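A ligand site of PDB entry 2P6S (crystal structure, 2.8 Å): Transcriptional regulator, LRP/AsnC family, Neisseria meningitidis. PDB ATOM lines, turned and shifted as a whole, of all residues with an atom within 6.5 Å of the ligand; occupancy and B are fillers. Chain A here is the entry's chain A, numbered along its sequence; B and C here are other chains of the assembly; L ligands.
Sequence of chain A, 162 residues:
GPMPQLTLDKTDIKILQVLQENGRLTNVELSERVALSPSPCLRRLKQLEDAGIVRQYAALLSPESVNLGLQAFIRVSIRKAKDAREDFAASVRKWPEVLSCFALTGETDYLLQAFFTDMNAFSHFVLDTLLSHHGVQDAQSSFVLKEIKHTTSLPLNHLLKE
The backbone carbonyl oxygen of Ala 139 of chain B sits close to an oxygen (O1) of the ligand, 3.3 Å away. CB of Ala 103 touches C5 of the ligand, 3.6 Å away. Thr 105 touches the ligand. CZ of Tyr 110 touches C5 of the ligand (3.7 Å). Val 126 of chain B touches the ligand (CG1 to O2, 3.8 Å). CD2 of Leu 127 of chain B touches S1 of the ligand (3.8 Å). Leu 131 of chain B touches the ligand (CD1 to S1, 3.5 Å). Gln 140 of chain B touches the ligand (CA to O1, 3.2 Å). CD1 of Leu 145 of chain C touches C3 of the ligand, at 3.97 Å. Hydrophobic or aromatic side chains within 4 Å of the ligand: Ala 103, Tyr 110, Val 126 of chain B, Leu 127 of chain B, Leu 131 of chain B and Leu 145 of chain C. Within 4 Å of the ligand: Ala 103, Leu 104, Thr 105, Gly 106, Thr 108, Asp 109, Tyr 110, Val 126 of chain B, Leu 127 of chain B, Leu 131 of chain B, Ala 139 of chain B, Gln 140 of chain B, Ser 141 of chain B and Leu 145 of chain C. The nearest printed residue that does not touch the ligand is Glu 107 (4.7 Å).
The backbone NH (N) of Ser 141 of chain B lies within hydrogen-bond range of an oxygen (O1) of the ligand, 2.9 Å away. The side-chain carboxylate (OD2) of Asp 109 lies within salt-bridge range of a nitrogen (N1) of the ligand, 3.2 Å away. O of Thr 108 sits at hydrogen-bond distance from N1 of the ligand (3.0 Å). The backbone NH (N) of Gly 106 lies within hydrogen-bond range of an oxygen (O1) of the ligand (2.6 Å). N1 of the ligand sits at hydrogen-bond distance from O of Gly 106 (2.7 Å). The backbone carbonyl oxygen (O) of Leu 104 sits at hydrogen-bond distance from a nitrogen (N1) of the ligand (2.9 Å). The side-chain hydroxyl (OG) of Ser 141 of chain B lies within hydrogen-bond range of an oxygen (O2) of the ligand (3.2 Å).
The backbone NH (N) of Leu 104 lies within hydrogen-bond range of the backbone carbonyl oxygen (O) of Asp 109 (3.2 Å). O of Tyr 110 is in hydrogen-bond range of OG1 of Thr 108. The backbone carbonyl oxygen (O) of Leu 127 of chain B sits at hydrogen-bond distance from the guanidinium group (NH1) of Arg 85, 3.1 Å away. N of Leu 145 of chain C lies within hydrogen-bond range of O of Ala 103 (2.7 Å). The backbone NH (N) of Leu 131 of chain B lies within hydrogen-bond range of the backbone carbonyl oxygen (O) of Val 126 of chain B (2.9 Å).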
ATOM      1  N   ARG A  85      23.689   0.387 -16.669  1.00  0.00           N
ATOM      2  CA  ARG A  85      22.647  -0.271 -15.876  1.00  0.00           C
ATOM      3  C   ARG A  85      21.404  -0.631 -16.699  1.00  0.00           C
ATOM      4  O   ARG A  85      20.909  -1.749 -16.620  1.00  0.00           O
ATOM      5  CB  ARG A  85      22.242   0.611 -14.676  1.00  0.00           C
ATOM      6  CG  ARG A  85      23.281   0.639 -13.553  1.00  0.00           C
ATOM      7  CD  ARG A  85      22.746   1.319 -12.292  1.00  0.00           C
ATOM      8  NE  ARG A  85      22.518   2.755 -12.488  1.00  0.00           N
ATOM      9  CZ  ARG A  85      21.985   3.578 -11.588  1.00  0.00           C
ATOM     10  NH1 ARG A  85      21.618   3.127 -10.400  1.00  0.00           N
ATOM     11  NH2 ARG A  85      21.831   4.868 -11.883  1.00  0.00           N
ATOM     12  N   PHE A 102      18.451  -9.215  -9.438  1.00  0.00           N
ATOM     13  CA  PHE A 102      18.207  -8.242  -8.379  1.00  0.00           C
ATOM     14  C   PHE A 102      19.392  -7.313  -8.150  1.00  0.00           C
ATOM     15  O   PHE A 102      20.535  -7.746  -8.156  1.00  0.00           O
ATOM     16  CB  PHE A 102      17.852  -8.969  -7.071  1.00  0.00           C
ATOM     17  CG  PHE A 102      16.639  -9.848  -7.185  1.00  0.00           C
ATOM     18  CD1 PHE A 102      15.363  -9.314  -7.163  1.00  0.00           C
ATOM     19  CD2 PHE A 102      16.772 -11.217  -7.357  1.00  0.00           C
ATOM     20  CE1 PHE A 102      14.260 -10.120  -7.290  1.00  0.00           C
ATOM     21  CE2 PHE A 102      15.668 -12.022  -7.484  1.00  0.00           C
ATOM     22  CZ  PHE A 102      14.411 -11.472  -7.461  1.00  0.00           C
ATOM     23  N   ALA A 103      19.088  -6.033  -7.949  1.00  0.00           N
ATOM     24  CA  ALA A 103      20.043  -5.079  -7.398  1.00  0.00           C
ATOM     25  C   ALA A 103      20.152  -5.309  -5.889  1.00  0.00           C
ATOM     26  O   ALA A 103      19.235  -4.954  -5.146  1.00  0.00           O
ATOM     27  CB  ALA A 103      19.571  -3.664  -7.685  1.00  0.00           C
ATOM     28  N   LEU A 104      21.257  -5.920  -5.439  1.00  0.00           N
ATOM     29  CA  LEU A 104      21.446  -6.201  -4.007  1.00  0.00           C
ATOM     30  C   LEU A 104      22.321  -5.167  -3.318  1.00  0.00           C
ATOM     31  O   LEU A 104      23.169  -4.530  -3.947  1.00  0.00           O
ATOM     32  CB  LEU A 104      22.102  -7.569  -3.781  1.00  0.00           C
ATOM     33  CG  LEU A 104      21.227  -8.822  -3.752  1.00  0.00           C
ATOM     34  CD1 LEU A 104      22.072  -9.987  -3.278  1.00  0.00           C
ATOM     35  CD2 LEU A 104      20.016  -8.631  -2.851  1.00  0.00           C
ATOM     36  N   THR A 105      22.135  -5.051  -2.006  1.00  0.00           N
ATOM     37  CA  THR A 105      23.051  -4.311  -1.167  1.00  0.00           C
ATOM     38  C   THR A 105      24.237  -5.226  -0.870  1.00  0.00           C
ATOM     39  O   THR A 105      24.141  -6.445  -1.056  1.00  0.00           O
ATOM     40  CB  THR A 105      22.400  -3.848   0.145  1.00  0.00           C
ATOM     41  OG1 THR A 105      22.157  -4.977   0.992  1.00  0.00           O
ATOM     42  CG2 THR A 105      21.093  -3.132  -0.134  1.00  0.00           C
ATOM     43  N   GLY A 106      25.349  -4.650  -0.414  1.00  0.00           N
ATOM     44  CA  GLY A 106      26.553  -5.418  -0.115  1.00  0.00           C
ATOM     45  C   GLY A 106      27.536  -5.519  -1.272  1.00  0.00           C
ATOM     46  O   GLY A 106      27.417  -4.786  -2.267  1.00  0.00           O
ATOM     47  N   GLU A 107      28.493  -6.444  -1.134  1.00  0.00           N
ATOM     48  CA  GLU A 107      29.662  -6.520  -2.030  1.00  0.00           C
ATOM     49  C   GLU A 107      29.279  -6.431  -3.491  1.00  0.00           C
ATOM     50  O   GLU A 107      29.877  -5.667  -4.242  1.00  0.00           O
ATOM     51  CB  GLU A 107      30.457  -7.810  -1.789  1.00  0.00           C
ATOM     52  CG  GLU A 107      31.373  -7.763  -0.560  1.00  0.00           C
ATOM     53  CD  GLU A 107      32.354  -8.924  -0.489  1.00  0.00           C
ATOM     54  OE1 GLU A 107      32.823  -9.228   0.638  1.00  0.00           O
ATOM     55  OE2 GLU A 107      32.656  -9.532  -1.534  1.00  0.00           O
ATOM     56  N   THR A 108      28.289  -7.218  -3.886  1.00  0.00           N
ATOM     57  CA  THR A 108      27.886  -7.292  -5.287  1.00  0.00           C
ATOM     58  C   THR A 108      26.740  -6.343  -5.575  1.00  0.00           C
ATOM     59  O   THR A 108      25.870  -6.105  -4.732  1.00  0.00           O
ATOM     60  CB  THR A 108      27.438  -8.717  -5.674  1.00  0.00           C
ATOM     61  OG1 THR A 108      26.125  -8.970  -5.154  1.00  0.00           O
ATOM     62  CG2 THR A 108      28.435  -9.736  -5.132  1.00  0.00           C
ATOM     63  N   ASP A 109      26.749  -5.825  -6.800  1.00  0.00           N
ATOM     64  CA  ASP A 109      25.726  -4.882  -7.242  1.00  0.00           C
ATOM     65  C   ASP A 109      24.499  -5.612  -7.814  1.00  0.00           C
ATOM     66  O   ASP A 109      23.372  -5.111  -7.710  1.00  0.00           O
ATOM     67  CB  ASP A 109      26.316  -3.920  -8.285  1.00  0.00           C
ATOM     68  CG  ASP A 109      27.475  -3.088  -7.738  1.00  0.00           C
ATOM     69  OD1 ASP A 109      28.352  -2.699  -8.556  1.00  0.00           O
ATOM     70  OD2 ASP A 109      27.518  -2.807  -6.504  1.00  0.00           O
ATOM     71  N   TYR A 110      24.719  -6.795  -8.402  1.00  0.00           N
ATOM     72  CA  TYR A 110      23.631  -7.599  -8.959  1.00  0.00           C
ATOM     73  C   TYR A 110      23.724  -9.082  -8.590  1.00  0.00           C
ATOM     74  O   TYR A 110      24.809  -9.592  -8.270  1.00  0.00           O
ATOM     75  CB  TYR A 110      23.558  -7.430 -10.481  1.00  0.00           C
ATOM     76  CG  TYR A 110      23.095  -6.045 -10.895  1.00  0.00           C
ATOM     77  CD1 TYR A 110      21.749  -5.750 -11.067  1.00  0.00           C
ATOM     78  CD2 TYR A 110      24.026  -5.029 -11.083  1.00  0.00           C
ATOM     79  CE1 TYR A 110      21.331  -4.483 -11.427  1.00  0.00           C
ATOM     80  CE2 TYR A 110      23.615  -3.758 -11.448  1.00  0.00           C
ATOM     81  CZ  TYR A 110      22.275  -3.481 -11.625  1.00  0.00           C
ATOM     82  OH  TYR A 110      21.899  -2.198 -11.988  1.00  0.00           O
ATOM     83  N   ILE B  74      26.873   3.068   5.145  1.00  0.00           N
ATOM     84  CA  ILE B  74      27.305   2.781   3.776  1.00  0.00           C
ATOM     85  C   ILE B  74      28.824   2.974   3.623  1.00  0.00           C
ATOM     86  O   ILE B  74      29.343   4.019   4.019  1.00  0.00           O
ATOM     87  CB  ILE B  74      26.587   3.688   2.760  1.00  0.00           C
ATOM     88  CG1 ILE B  74      25.091   3.702   3.033  1.00  0.00           C
ATOM     89  CG2 ILE B  74      26.835   3.203   1.356  1.00  0.00           C
ATOM     90  CD1 ILE B  74      24.291   4.425   1.986  1.00  0.00           C
ATOM     91  N   PHE B 122      15.506   4.085   0.549  1.00  0.00           N
ATOM     92  CA  PHE B 122      16.938   3.883   0.509  1.00  0.00           C
ATOM     93  C   PHE B 122      17.431   3.515  -0.889  1.00  0.00           C
ATOM     94  O   PHE B 122      18.522   3.912  -1.297  1.00  0.00           O
ATOM     95  CB  PHE B 122      17.343   2.813   1.516  1.00  0.00           C
ATOM     96  CG  PHE B 122      18.784   2.425   1.444  1.00  0.00           C
ATOM     97  CD1 PHE B 122      19.753   3.223   2.033  1.00  0.00           C
ATOM     98  CD2 PHE B 122      19.188   1.284   0.771  1.00  0.00           C
ATOM     99  CE1 PHE B 122      21.074   2.878   1.970  1.00  0.00           C
ATOM    100  CE2 PHE B 122      20.511   0.944   0.695  1.00  0.00           C
ATOM    101  CZ  PHE B 122      21.458   1.739   1.309  1.00  0.00           C
ATOM    102  N   VAL B 126      20.303   5.332  -3.162  1.00  0.00           N
ATOM    103  CA  VAL B 126      21.513   4.600  -3.538  1.00  0.00           C
ATOM    104  C   VAL B 126      21.647   4.513  -5.044  1.00  0.00           C
ATOM    105  O   VAL B 126      22.739   4.682  -5.587  1.00  0.00           O
ATOM    106  CB  VAL B 126      21.541   3.195  -2.909  1.00  0.00           C
ATOM    107  CG1 VAL B 126      22.709   2.393  -3.462  1.00  0.00           C
ATOM    108  CG2 VAL B 126      21.641   3.310  -1.402  1.00  0.00           C
ATOM    109  N   LEU B 127      20.541   4.266  -5.728  1.00  0.00           N
ATOM    110  CA  LEU B 127      20.550   4.142  -7.176  1.00  0.00           C
ATOM    111  C   LEU B 127      20.657   5.508  -7.847  1.00  0.00           C
ATOM    112  O   LEU B 127      21.553   5.730  -8.667  1.00  0.00           O
ATOM    113  CB  LEU B 127      19.289   3.421  -7.654  1.00  0.00           C
ATOM    114  CG  LEU B 127      19.198   1.941  -7.246  1.00  0.00           C
ATOM    115  CD1 LEU B 127      17.743   1.492  -7.113  1.00  0.00           C
ATOM    116  CD2 LEU B 127      19.938   1.064  -8.248  1.00  0.00           C
ATOM    117  N   LEU B 130      23.588   8.348  -4.883  1.00  0.00           N
ATOM    118  CA  LEU B 130      24.941   7.946  -4.488  1.00  0.00           C
ATOM    119  C   LEU B 130      25.702   7.288  -5.645  1.00  0.00           C
ATOM    120  O   LEU B 130      26.771   7.773  -6.038  1.00  0.00           O
ATOM    121  CB  LEU B 130      24.889   6.986  -3.297  1.00  0.00           C
ATOM    122  CG  LEU B 130      26.248   6.539  -2.750  1.00  0.00           C
ATOM    123  CD1 LEU B 130      27.043   7.742  -2.247  1.00  0.00           C
ATOM    124  CD2 LEU B 130      26.073   5.502  -1.648  1.00  0.00           C
ATOM    125  N   LEU B 131      25.153   6.201  -6.179  1.00  0.00           N
ATOM    126  CA  LEU B 131      25.806   5.453  -7.254  1.00  0.00           C
ATOM    127  C   LEU B 131      25.785   6.175  -8.602  1.00  0.00           C
ATOM    128  O   LEU B 131      26.543   5.825  -9.504  1.00  0.00           O
ATOM    129  CB  LEU B 131      25.175   4.058  -7.400  1.00  0.00           C
ATOM    130  CG  LEU B 131      25.320   3.082  -6.220  1.00  0.00           C
ATOM    131  CD1 LEU B 131      24.442   1.868  -6.441  1.00  0.00           C
ATOM    132  CD2 LEU B 131      26.764   2.667  -5.993  1.00  0.00           C
ATOM    133  N   ASP B 138      31.941   2.619  -6.103  1.00  0.00           N
ATOM    134  CA  ASP B 138      31.220   1.458  -5.551  1.00  0.00           C
ATOM    135  C   ASP B 138      30.754   1.708  -4.124  1.00  0.00           C
ATOM    136  O   ASP B 138      31.477   2.314  -3.327  1.00  0.00           O
ATOM    137  CB  ASP B 138      32.115   0.195  -5.592  1.00  0.00           C
ATOM    138  CG  ASP B 138      31.312  -1.098  -5.466  1.00  0.00           C
ATOM    139  OD1 ASP B 138      30.060  -1.080  -5.572  1.00  0.00           O
ATOM    140  OD2 ASP B 138      31.939  -2.166  -5.267  1.00  0.00           O
ATOM    141  N   ALA B 139      29.550   1.225  -3.798  1.00  0.00           N
ATOM    142  CA  ALA B 139      28.969   1.368  -2.452  1.00  0.00           C
ATOM    143  C   ALA B 139      28.616   0.008  -1.893  1.00  0.00           C
ATOM    144  O   ALA B 139      28.278  -0.899  -2.637  1.00  0.00           O
ATOM    145  CB  ALA B 139      27.739   2.256  -2.480  1.00  0.00           C
ATOM    146  N   GLN B 140      28.705  -0.132  -0.561  1.00  0.00           N
ATOM    147  CA  GLN B 140      28.320  -1.347   0.164  1.00  0.00           C
ATOM    148  C   GLN B 140      27.503  -0.949   1.369  1.00  0.00           C
ATOM    149  O   GLN B 140      28.040  -0.432   2.349  1.00  0.00           O
ATOM    150  CB  GLN B 140      29.556  -2.089   0.670  1.00  0.00           C
ATOM    151  CG  GLN B 140      30.422  -2.700  -0.390  1.00  0.00           C
ATOM    152  CD  GLN B 140      31.557  -3.510   0.206  1.00  0.00           C
ATOM    153  OE1 GLN B 140      31.844  -3.404   1.397  1.00  0.00           O
ATOM    154  NE2 GLN B 140      32.206  -4.319  -0.627  1.00  0.00           N
ATOM    155  N   SER B 141      26.199  -1.208   1.344  1.00  0.00           N
ATOM    156  CA  SER B 141      25.344  -0.762   2.430  1.00  0.00           C
ATOM    157  C   SER B 141      24.965  -1.849   3.441  1.00  0.00           C
ATOM    158  O   SER B 141      24.467  -2.916   3.078  1.00  0.00           O
ATOM    159  CB  SER B 141      24.089  -0.151   1.852  1.00  0.00           C
ATOM    160  OG  SER B 141      24.455   0.955   1.055  1.00  0.00           O
ATOM    161  N   SER B 142      25.206  -1.550   4.711  1.00  0.00           N
ATOM    162  CA  SER B 142      24.741  -2.374   5.816  1.00  0.00           C
ATOM    163  C   SER B 142      23.732  -1.578   6.625  1.00  0.00           C
ATOM    164  O   SER B 142      23.768  -0.362   6.599  1.00  0.00           O
ATOM    165  CB  SER B 142      25.921  -2.762   6.711  1.00  0.00           C
ATOM    166  OG  SER B 142      25.682  -4.024   7.302  1.00  0.00           O
ATOM    167  N   LEU C 145      17.069  -3.931  -3.820  1.00  0.00           N
ATOM    168  CA  LEU C 145      16.785  -2.515  -4.016  1.00  0.00           C
ATOM    169  C   LEU C 145      15.956  -2.262  -5.276  1.00  0.00           C
ATOM    170  O   LEU C 145      15.242  -1.254  -5.357  1.00  0.00           O
ATOM    171  CB  LEU C 145      18.101  -1.725  -4.054  1.00  0.00           C
ATOM    172  CG  LEU C 145      18.961  -1.786  -2.777  1.00  0.00           C
ATOM    173  CD1 LEU C 145      20.386  -1.339  -3.034  1.00  0.00           C
ATOM    174  CD2 LEU C 145      18.325  -0.956  -1.652  1.00  0.00           C
HETATM  175  N1  LIG L   1      25.780  -3.241  -3.844  1.00  0.00           N
HETATM  176  C1  LIG L   1      25.401  -1.800  -3.652  1.00  0.00           C
HETATM  177  C2  LIG L   1      25.227  -1.447  -2.178  1.00  0.00           C
HETATM  178  O1  LIG L   1      25.577  -2.217  -1.277  1.00  0.00           O
HETATM  179  C3  LIG L   1      24.108  -1.474  -4.411  1.00  0.00           C
HETATM  180  C4  LIG L   1      24.117  -1.845  -5.873  1.00  0.00           C
HETATM  181  S1  LIG L   1      22.723  -1.122  -6.754  1.00  0.00           S
HETATM  182  C5  LIG L   1      22.772  -2.026  -8.294  1.00  0.00           C
HETATM  183  O2  LIG L   1      24.720  -0.372  -1.832  1.00  0.00           O
